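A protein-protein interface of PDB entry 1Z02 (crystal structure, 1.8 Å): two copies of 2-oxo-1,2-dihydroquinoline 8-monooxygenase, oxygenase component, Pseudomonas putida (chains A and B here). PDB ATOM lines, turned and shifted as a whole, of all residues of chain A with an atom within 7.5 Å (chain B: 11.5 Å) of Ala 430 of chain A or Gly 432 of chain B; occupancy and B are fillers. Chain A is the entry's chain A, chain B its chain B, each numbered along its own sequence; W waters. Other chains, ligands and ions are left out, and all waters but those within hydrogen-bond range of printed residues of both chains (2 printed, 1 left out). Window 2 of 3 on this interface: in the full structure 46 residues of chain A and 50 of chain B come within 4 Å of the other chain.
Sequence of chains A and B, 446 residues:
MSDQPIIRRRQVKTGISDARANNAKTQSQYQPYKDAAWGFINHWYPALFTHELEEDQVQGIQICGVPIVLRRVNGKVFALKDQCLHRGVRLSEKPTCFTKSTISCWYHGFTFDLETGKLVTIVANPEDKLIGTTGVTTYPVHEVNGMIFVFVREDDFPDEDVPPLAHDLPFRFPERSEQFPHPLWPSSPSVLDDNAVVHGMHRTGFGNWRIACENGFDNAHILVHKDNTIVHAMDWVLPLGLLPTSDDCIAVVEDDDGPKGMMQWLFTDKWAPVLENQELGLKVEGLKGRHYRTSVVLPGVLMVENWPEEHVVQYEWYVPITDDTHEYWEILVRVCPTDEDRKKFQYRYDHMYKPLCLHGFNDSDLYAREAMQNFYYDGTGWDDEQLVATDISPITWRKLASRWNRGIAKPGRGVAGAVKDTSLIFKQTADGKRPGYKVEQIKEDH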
ATOM      1  N   LEU A 424       8.103  13.765 -29.797  1.00  0.00           N
ATOM      2  CA  LEU A 424       7.612  12.386 -29.789  1.00  0.00           C
ATOM      3  C   LEU A 424       8.170  11.648 -28.576  1.00  0.00           C
ATOM      4  O   LEU A 424       7.455  10.879 -27.919  1.00  0.00           O
ATOM      5  CB  LEU A 424       8.051  11.631 -31.045  1.00  0.00           C
ATOM      6  CG  LEU A 424       7.156  11.766 -32.278  1.00  0.00           C
ATOM      7  CD1 LEU A 424       7.842  11.114 -33.481  1.00  0.00           C
ATOM      8  CD2 LEU A 424       5.804  11.122 -31.990  1.00  0.00           C
ATOM      9  N   ILE A 425       9.454  11.861 -28.297  1.00  0.00           N
ATOM     10  CA  ILE A 425      10.076  11.214 -27.154  1.00  0.00           C
ATOM     11  C   ILE A 425       9.468  11.757 -25.869  1.00  0.00           C
ATOM     12  O   ILE A 425       9.241  10.990 -24.937  1.00  0.00           O
ATOM     13  CB  ILE A 425      11.602  11.397 -27.169  1.00  0.00           C
ATOM     14  CG1 ILE A 425      12.192  10.548 -28.294  1.00  0.00           C
ATOM     15  CG2 ILE A 425      12.206  10.991 -25.832  1.00  0.00           C
ATOM     16  CD1 ILE A 425      13.665  10.758 -28.545  1.00  0.00           C
ATOM     17  N   PHE A 426       9.182  13.061 -25.809  1.00  0.00           N
ATOM     18  CA  PHE A 426       8.566  13.622 -24.602  1.00  0.00           C
ATOM     19  C   PHE A 426       7.131  13.113 -24.444  1.00  0.00           C
ATOM     20  O   PHE A 426       6.639  12.939 -23.320  1.00  0.00           O
ATOM     21  CB  PHE A 426       8.580  15.158 -24.619  1.00  0.00           C
ATOM     22  CG  PHE A 426       9.899  15.755 -24.211  1.00  0.00           C
ATOM     23  CD1 PHE A 426      10.753  16.314 -25.162  1.00  0.00           C
ATOM     24  CD2 PHE A 426      10.301  15.738 -22.874  1.00  0.00           C
ATOM     25  CE1 PHE A 426      11.982  16.849 -24.781  1.00  0.00           C
ATOM     26  CE2 PHE A 426      11.531  16.270 -22.480  1.00  0.00           C
ATOM     27  CZ  PHE A 426      12.373  16.823 -23.429  1.00  0.00           C
ATOM     28  N   LYS A 427       6.451  12.882 -25.563  1.00  0.00           N
ATOM     29  CA  LYS A 427       5.090  12.346 -25.504  1.00  0.00           C
ATOM     30  C   LYS A 427       5.150  10.947 -24.881  1.00  0.00           C
ATOM     31  O   LYS A 427       4.411  10.626 -23.953  1.00  0.00           O
ATOM     32  CB  LYS A 427       4.490  12.220 -26.905  1.00  0.00           C
ATOM     33  CG  LYS A 427       3.144  11.502 -26.934  1.00  0.00           C
ATOM     34  CD  LYS A 427       2.797  10.983 -28.319  1.00  0.00           C
ATOM     35  CE  LYS A 427       1.430  10.294 -28.309  1.00  0.00           C
ATOM     36  NZ  LYS A 427       0.980   9.761 -29.638  1.00  0.00           N
ATOM     37  N   GLN A 428       6.043  10.119 -25.407  1.00  0.00           N
ATOM     38  CA  GLN A 428       6.203   8.761 -24.918  1.00  0.00           C
ATOM     39  C   GLN A 428       6.593   8.734 -23.455  1.00  0.00           C
ATOM     40  O   GLN A 428       6.065   7.931 -22.686  1.00  0.00           O
ATOM     41  CB  GLN A 428       7.267   8.033 -25.734  1.00  0.00           C
ATOM     42  CG  GLN A 428       6.934   7.915 -27.206  1.00  0.00           C
ATOM     43  CD  GLN A 428       8.018   7.204 -27.999  1.00  0.00           C
ATOM     44  OE1 GLN A 428       7.891   7.015 -29.212  1.00  0.00           O
ATOM     45  NE2 GLN A 428       9.090   6.807 -27.317  1.00  0.00           N
ATOM     46  N   THR A 429       7.526   9.607 -23.083  1.00  0.00           N
ATOM     47  CA  THR A 429       8.001   9.687 -21.706  1.00  0.00           C
ATOM     48  C   THR A 429       6.873  10.113 -20.787  1.00  0.00           C
ATOM     49  O   THR A 429       6.723   9.577 -19.692  1.00  0.00           O
ATOM     50  CB  THR A 429       9.151  10.685 -21.575  1.00  0.00           C
ATOM     51  OG1 THR A 429      10.116  10.416 -22.597  1.00  0.00           O
ATOM     52  CG2 THR A 429       9.828  10.564 -20.222  1.00  0.00           C
ATOM     53  N   ALA A 430       6.082  11.079 -21.239  1.00  0.00           N
ATOM     54  CA  ALA A 430       4.947  11.565 -20.454  1.00  0.00           C
ATOM     55  C   ALA A 430       3.962  10.430 -20.209  1.00  0.00           C
ATOM     56  O   ALA A 430       3.313  10.370 -19.162  1.00  0.00           O
ATOM     57  CB  ALA A 430       4.251  12.691 -21.189  1.00  0.00           C
ATOM     58  N   ASP A 431       3.844   9.543 -21.192  1.00  0.00           N
ATOM     59  CA  ASP A 431       2.948   8.389 -21.104  1.00  0.00           C
ATOM     60  C   ASP A 431       3.517   7.279 -20.231  1.00  0.00           C
ATOM     61  O   ASP A 431       2.867   6.262 -20.021  1.00  0.00           O
ATOM     62  CB  ASP A 431       2.650   7.831 -22.500  1.00  0.00           C
ATOM     63  CG  ASP A 431       1.774   8.756 -23.324  1.00  0.00           C
ATOM     64  OD1 ASP A 431       1.562   8.452 -24.515  1.00  0.00           O
ATOM     65  OD2 ASP A 431       1.298   9.782 -22.792  1.00  0.00           O
ATOM     66  N   GLY A 432       4.730   7.474 -19.724  1.00  0.00           N
ATOM     67  CA  GLY A 432       5.336   6.475 -18.864  1.00  0.00           C
ATOM     68  C   GLY A 432       6.218   5.456 -19.566  1.00  0.00           C
ATOM     69  O   GLY A 432       6.665   4.497 -18.938  1.00  0.00           O
ATOM     70  N   LYS A 433       6.477   5.653 -20.856  1.00  0.00           N
ATOM     71  CA  LYS A 433       7.307   4.718 -21.621  1.00  0.00           C
ATOM     72  C   LYS A 433       8.787   5.040 -21.565  1.00  0.00           C
ATOM     73  O   LYS A 433       9.200   6.135 -21.936  1.00  0.00           O
ATOM     74  CB  LYS A 433       6.876   4.700 -23.083  1.00  0.00           C
ATOM     75  CG  LYS A 433       5.526   4.090 -23.303  1.00  0.00           C
ATOM     76  CD  LYS A 433       5.114   4.174 -24.751  1.00  0.00           C
ATOM     77  CE  LYS A 433       4.005   3.177 -25.003  1.00  0.00           C
ATOM     78  NZ  LYS A 433       3.044   3.609 -26.040  1.00  0.00           N
ATOM     79  N   THR B 204      -3.449  18.525 -30.358  1.00  0.00           N
ATOM     80  CA  THR B 204      -2.029  18.773 -30.560  1.00  0.00           C
ATOM     81  C   THR B 204      -1.436  17.555 -31.263  1.00  0.00           C
ATOM     82  O   THR B 204      -1.746  16.413 -30.907  1.00  0.00           O
ATOM     83  CB  THR B 204      -1.317  18.985 -29.218  1.00  0.00           C
ATOM     84  OG1 THR B 204      -1.919  20.097 -28.539  1.00  0.00           O
ATOM     85  CG2 THR B 204       0.170  19.262 -29.434  1.00  0.00           C
ATOM     86  N   PHE B 206       2.095  15.505 -32.553  1.00  0.00           N
ATOM     87  CA  PHE B 206       3.510  15.430 -32.206  1.00  0.00           C
ATOM     88  C   PHE B 206       4.361  15.232 -33.454  1.00  0.00           C
ATOM     89  O   PHE B 206       4.439  14.148 -34.016  1.00  0.00           O
ATOM     90  CB  PHE B 206       3.707  14.330 -31.166  1.00  0.00           C
ATOM     91  CG  PHE B 206       2.784  14.484 -29.996  1.00  0.00           C
ATOM     92  CD1 PHE B 206       1.555  13.832 -29.980  1.00  0.00           C
ATOM     93  CD2 PHE B 206       3.071  15.400 -28.982  1.00  0.00           C
ATOM     94  CE1 PHE B 206       0.616  14.086 -28.992  1.00  0.00           C
ATOM     95  CE2 PHE B 206       2.130  15.665 -27.980  1.00  0.00           C
ATOM     96  CZ  PHE B 206       0.899  15.008 -27.986  1.00  0.00           C
ATOM     97  N   THR B 325       5.821  20.528 -33.107  1.00  0.00           N
ATOM     98  CA  THR B 325       4.455  20.290 -32.642  1.00  0.00           C
ATOM     99  C   THR B 325       3.521  21.192 -33.445  1.00  0.00           C
ATOM    100  O   THR B 325       3.913  22.261 -33.918  1.00  0.00           O
ATOM    101  CB  THR B 325       4.246  20.582 -31.114  1.00  0.00           C
ATOM    102  OG1 THR B 325       4.618  21.935 -30.807  1.00  0.00           O
ATOM    103  CG2 THR B 325       5.047  19.610 -30.272  1.00  0.00           C
ATOM    104  N   SER B 423      14.355  22.029 -17.315  1.00  0.00           N
ATOM    105  CA  SER B 423      13.943  21.247 -16.159  1.00  0.00           C
ATOM    106  C   SER B 423      12.429  21.400 -15.990  1.00  0.00           C
ATOM    107  O   SER B 423      11.783  20.530 -15.414  1.00  0.00           O
ATOM    108  CB  SER B 423      14.663  21.720 -14.893  1.00  0.00           C
ATOM    109  OG  SER B 423      14.356  23.069 -14.593  1.00  0.00           O
ATOM    110  N   LEU B 424      11.868  22.505 -16.483  1.00  0.00           N
ATOM    111  CA  LEU B 424      10.425  22.724 -16.412  1.00  0.00           C
ATOM    112  C   LEU B 424       9.701  21.686 -17.269  1.00  0.00           C
ATOM    113  O   LEU B 424       8.696  21.116 -16.850  1.00  0.00           O
ATOM    114  CB  LEU B 424      10.070  24.120 -16.909  1.00  0.00           C
ATOM    115  CG  LEU B 424      10.072  25.258 -15.897  1.00  0.00           C
ATOM    116  CD1 LEU B 424       9.919  26.574 -16.639  1.00  0.00           C
ATOM    117  CD2 LEU B 424       8.925  25.059 -14.897  1.00  0.00           C
ATOM    118  N   ILE B 425      10.215  21.449 -18.472  1.00  0.00           N
ATOM    119  CA  ILE B 425       9.616  20.460 -19.359  1.00  0.00           C
ATOM    120  C   ILE B 425       9.779  19.036 -18.801  1.00  0.00           C
ATOM    121  O   ILE B 425       8.863  18.224 -18.922  1.00  0.00           O
ATOM    122  CB  ILE B 425      10.196  20.582 -20.803  1.00  0.00           C
ATOM    123  CG1 ILE B 425       9.589  21.819 -21.481  1.00  0.00           C
ATOM    124  CG2 ILE B 425       9.878  19.333 -21.624  1.00  0.00           C
ATOM    125  CD1 ILE B 425      10.270  22.228 -22.779  1.00  0.00           C
ATOM    126  N   PHE B 426      10.911  18.733 -18.162  1.00  0.00           N
ATOM    127  CA  PHE B 426      11.084  17.396 -17.594  1.00  0.00           C
ATOM    128  C   PHE B 426      10.153  17.203 -16.406  1.00  0.00           C
ATOM    129  O   PHE B 426       9.661  16.092 -16.154  1.00  0.00           O
ATOM    130  CB  PHE B 426      12.541  17.140 -17.179  1.00  0.00           C
ATOM    131  CG  PHE B 426      13.426  16.719 -18.320  1.00  0.00           C
ATOM    132  CD1 PHE B 426      14.382  17.581 -18.835  1.00  0.00           C
ATOM    133  CD2 PHE B 426      13.293  15.451 -18.883  1.00  0.00           C
ATOM    134  CE1 PHE B 426      15.196  17.191 -19.895  1.00  0.00           C
ATOM    135  CE2 PHE B 426      14.101  15.051 -19.943  1.00  0.00           C
ATOM    136  CZ  PHE B 426      15.054  15.921 -20.452  1.00  0.00           C
ATOM    137  N   LYS B 427       9.894  18.292 -15.687  1.00  0.00           N
ATOM    138  CA  LYS B 427       9.003  18.255 -14.531  1.00  0.00           C
ATOM    139  C   LYS B 427       7.592  17.911 -14.990  1.00  0.00           C
ATOM    140  O   LYS B 427       6.941  17.050 -14.411  1.00  0.00           O
ATOM    141  CB  LYS B 427       8.963  19.613 -13.830  1.00  0.00           C
ATOM    142  CG  LYS B 427       7.894  19.698 -12.761  1.00  0.00           C
ATOM    143  CD  LYS B 427       7.421  21.123 -12.581  1.00  0.00           C
ATOM    144  CE  LYS B 427       6.363  21.192 -11.508  1.00  0.00           C
ATOM    145  NZ  LYS B 427       5.842  22.578 -11.339  1.00  0.00           N
ATOM    146  N   GLN B 428       7.130  18.600 -16.030  1.00  0.00           N
ATOM    147  CA  GLN B 428       5.798  18.385 -16.583  1.00  0.00           C
ATOM    148  C   GLN B 428       5.658  16.978 -17.151  1.00  0.00           C
ATOM    149  O   GLN B 428       4.632  16.321 -16.964  1.00  0.00           O
ATOM    150  CB  GLN B 428       5.520  19.400 -17.687  1.00  0.00           C
ATOM    151  CG  GLN B 428       5.528  20.836 -17.216  1.00  0.00           C
ATOM    152  CD  GLN B 428       5.394  21.829 -18.362  1.00  0.00           C
ATOM    153  OE1 GLN B 428       5.343  23.042 -18.147  1.00  0.00           O
ATOM    154  NE2 GLN B 428       5.339  21.318 -19.584  1.00  0.00           N
ATOM    155  N   THR B 429       6.695  16.529 -17.852  1.00  0.00           N
ATOM    156  CA  THR B 429       6.709  15.202 -18.459  1.00  0.00           C
ATOM    157  C   THR B 429       6.673  14.151 -17.347  1.00  0.00           C
ATOM    158  O   THR B 429       5.924  13.171 -17.431  1.00  0.00           O
ATOM    159  CB  THR B 429       7.977  15.012 -19.335  1.00  0.00           C
ATOM    160  OG1 THR B 429       8.101  16.122 -20.243  1.00  0.00           O
ATOM    161  CG2 THR B 429       7.881  13.719 -20.147  1.00  0.00           C
ATOM    162  N   ALA B 430       7.469  14.356 -16.303  1.00  0.00           N
ATOM    163  CA  ALA B 430       7.502  13.442 -15.155  1.00  0.00           C
ATOM    164  C   ALA B 430       6.102  13.299 -14.550  1.00  0.00           C
ATOM    165  O   ALA B 430       5.707  12.211 -14.132  1.00  0.00           O
ATOM    166  CB  ALA B 430       8.480  13.974 -14.092  1.00  0.00           C
ATOM    167  N   ASP B 431       5.370  14.414 -14.497  1.00  0.00           N
ATOM    168  CA  ASP B 431       4.002  14.452 -13.967  1.00  0.00           C
ATOM    169  C   ASP B 431       2.982  13.852 -14.945  1.00  0.00           C
ATOM    170  O   ASP B 431       1.795  13.795 -14.637  1.00  0.00           O
ATOM    171  CB  ASP B 431       3.593  15.899 -13.644  1.00  0.00           C
ATOM    172  CG  ASP B 431       4.354  16.484 -12.450  1.00  0.00           C
ATOM    173  OD1 ASP B 431       4.197  17.692 -12.189  1.00  0.00           O
ATOM    174  OD2 ASP B 431       5.099  15.747 -11.768  1.00  0.00           O
ATOM    175  N   GLY B 432       3.445  13.424 -16.120  1.00  0.00           N
ATOM    176  CA  GLY B 432       2.552  12.822 -17.096  1.00  0.00           C
ATOM    177  C   GLY B 432       1.942  13.759 -18.128  1.00  0.00           C
ATOM    178  O   GLY B 432       1.027  13.370 -18.854  1.00  0.00           O
ATOM    179  N   LYS B 433       2.433  14.992 -18.215  1.00  0.00           N
ATOM    180  CA  LYS B 433       1.892  15.942 -19.192  1.00  0.00           C
ATOM    181  C   LYS B 433       2.643  15.969 -20.507  1.00  0.00           C
ATOM    182  O   LYS B 433       3.840  16.257 -20.541  1.00  0.00           O
ATOM    183  CB  LYS B 433       1.886  17.359 -18.634  1.00  0.00           C
ATOM    184  CG  LYS B 433       0.898  17.568 -17.543  1.00  0.00           C
ATOM    185  CD  LYS B 433       1.078  18.916 -16.902  1.00  0.00           C
ATOM    186  CE  LYS B 433       0.104  19.029 -15.749  1.00  0.00           C
ATOM    187  NZ  LYS B 433       0.391  20.148 -14.822  1.00  0.00           N
ATOM    188  N   ARG B 434       1.921  15.689 -21.586  1.00  0.00           N
ATOM    189  CA  ARG B 434       2.490  15.694 -22.926  1.00  0.00           C
ATOM    190  C   ARG B 434       2.632  17.114 -23.448  1.00  0.00           C
ATOM    191  O   ARG B 434       2.052  18.048 -22.892  1.00  0.00           O
ATOM    192  CB  ARG B 434       1.566  14.970 -23.901  1.00  0.00           C
ATOM    193  CG  ARG B 434       1.275  13.536 -23.612  1.00  0.00           C
ATOM    194  CD  ARG B 434       0.156  13.097 -24.541  1.00  0.00           C
ATOM    195  NE  ARG B 434       0.167  11.664 -24.794  1.00  0.00           N
ATOM    196  CZ  ARG B 434      -0.623  11.057 -25.669  1.00  0.00           C
ATOM    197  NH1 ARG B 434      -0.537   9.743 -25.848  1.00  0.00           N
ATOM    198  NH2 ARG B 434      -1.510  11.767 -26.357  1.00  0.00           N
ATOM    199  N   PRO B 435       3.423  17.303 -24.516  1.00  0.00           N
ATOM    200  CA  PRO B 435       3.568  18.653 -25.067  1.00  0.00           C
ATOM    201  C   PRO B 435       2.147  19.099 -25.436  1.00  0.00           C
ATOM    202  O   PRO B 435       1.340  18.276 -25.867  1.00  0.00           O
ATOM    203  CB  PRO B 435       4.434  18.415 -26.290  1.00  0.00           C
ATOM    204  CG  PRO B 435       5.351  17.321 -25.805  1.00  0.00           C
ATOM    205  CD  PRO B 435       4.400  16.376 -25.125  1.00  0.00           C
ATOM    206  N   GLY B 436       1.834  20.381 -25.281  1.00  0.00           N
ATOM    207  CA  GLY B 436       0.480  20.813 -25.584  1.00  0.00           C
ATOM    208  C   GLY B 436       0.274  22.081 -26.394  1.00  0.00           C
ATOM    209  O   GLY B 436       1.132  22.486 -27.179  1.00  0.00           O
ATOM    210  N   GLU B 440      -1.761  26.125 -19.502  1.00  0.00           N
ATOM    211  CA  GLU B 440      -2.407  25.714 -18.264  1.00  0.00           C
ATOM    212  C   GLU B 440      -2.453  26.909 -17.327  1.00  0.00           C
ATOM    213  O   GLU B 440      -1.461  27.628 -17.174  1.00  0.00           O
ATOM    214  CB  GLU B 440      -1.620  24.580 -17.618  1.00  0.00           C
ATOM    215  CG  GLU B 440      -2.458  23.637 -16.789  1.00  0.00           C
ATOM    216  CD  GLU B 440      -1.616  22.604 -16.070  1.00  0.00           C
ATOM    217  OE1 GLU B 440      -2.179  21.597 -15.603  1.00  0.00           O
ATOM    218  OE2 GLU B 440      -0.387  22.798 -15.962  1.00  0.00           O
HETATM  219  O   HOH W   1      -1.994  10.227 -29.182  1.00  0.00           O
HETATM  220  O   HOH W   2       0.173  11.128 -20.848  1.00  0.00           O
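The side-chain carboxylate (OD1) of Asp 431 of chain A lies within salt-bridge range of the guanidinium group (NH1) of Arg 434 of chain B, 2.8 Å away.
The backbone carbonyl oxygen (O) of Ile 425 of chain A lies within hydrogen-bond range of the side-chain hydroxyl (OG1) of Thr 429 of chain A. OG1 of Thr 429 of chain B sits at hydrogen-bond distance from O of Ile 425 of chain B (2.6 Å). The backbone carbonyl oxygen of Gln 428 of chain B lies within hydrogen-bond range of the backbone NH of Lys 433 of chain B (2.9 Å). The side-chain amino group of Lys 433 of chain B lies within salt-bridge range of the side-chain carboxylate of Glu 440 of chain B, 3.0 Å away.
Leu 424 of chain A touches Phe 206 of chain B (CD2 to O, 3.9 Å). CG2 of Ile 425 of chain B touches CE2 of Phe 426 of chain A, 3.6 Å away. Phe 426 of chain B touches Phe 426 of chain A (CE2 to CE2, 3.8 Å). Phe 426 of chain A touches Thr 429 of chain B. Lys 427 of chain A touches Phe 206 of chain B. Lys 427 of chain A touches Arg 434 of chain B (CE to NH1, 3.2 Å). CB of Thr 429 of chain A touches CG2 of Thr 429 of chain B, at 3.6 Å. Ala 430 of chain A touches Gly 432 of chain B (O to CA, 3.3 Å). O of Lys 433 of chain B touches CB of Ala 430 of chain A, at 3.6 Å. N of Arg 434 of chain B touches CB of Ala 430 of chain A, at 3.8 Å.
Printed residues of chain B within 4 Å of Ala 430 of chain A: Thr 429 (3.4 Å), Gly 432 (3.3 Å), Lys 433 (3.6 Å) and Arg 434 (3.8 Å). Of the printed residues of chain A, Gly 432 of chain B touches Ala 430 (3.3 Å). Thr 429 of chain A touches one residue of chain B. Of chain B, only Arg 434 comes within 4 Å of Asp 431 of chain A. Gly 432 of chain A touches none of the printed residues of chain B. Printed residues of chain A within 4 Å of Phe 426 of chain B: Phe 426 (3.8 Å). Printed residues of chain B within 4 Å of Lys 427 of chain A: Phe 206 (3.5 Å) and Arg 434 (3.2 Å). Of the printed residues of chain A, Phe 206 of chain B touches Leu 424 and Lys 427. Glu 440 of chain B touches none of the printed residues of chain A. The nearest residue of chain B that does not touch Ala 430 of chain A is Pro 435 of chain B (5.4 Å). The nearest residue of chain A that does not touch Gly 432 of chain B is Asp 431 of chain A (5.3 Å).
Among the printed residues, Asp or Glu carboxylates within 4 Å of a Lys or Arg side-chain nitrogen of the other chain: Asp 431 of chain A with Arg 434 of chain B (2.8 Å).
Phe 426 of chain A touches Ile 425 of chain B, but with the chains exchanged Ile 425 of chain A does not touch Phe 426 of chain B (7.4 Å). Phe 426 of chain A touches Thr 429 of chain B, but with the chains exchanged Thr 429 of chain A does not touch Phe 426 of chain B (6.1 Å). Ala 430 of chain A touches Thr 429 of chain B, but with the chains exchanged Thr 429 of chain A does not touch Ala 430 of chain B (5.9 Å). Ala 430 of chain A touches Lys 433 of chain B, but with the chains exchanged Lys 433 of chain A does not touch Ala 430 of chain B (9.4 Å). Of the 12 pairs that touch across the chains among the printed residues, 2 have their exchanged pair printed and touching as well.
Water W2 bridges OD2 of Asp 431 of chain A (2.6 Å) and O of Gly 432 of chain B (3.1 Å). Water W1 bridges NZ of Lys 427 of chain A and NH2 of Arg 434 of chain B.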
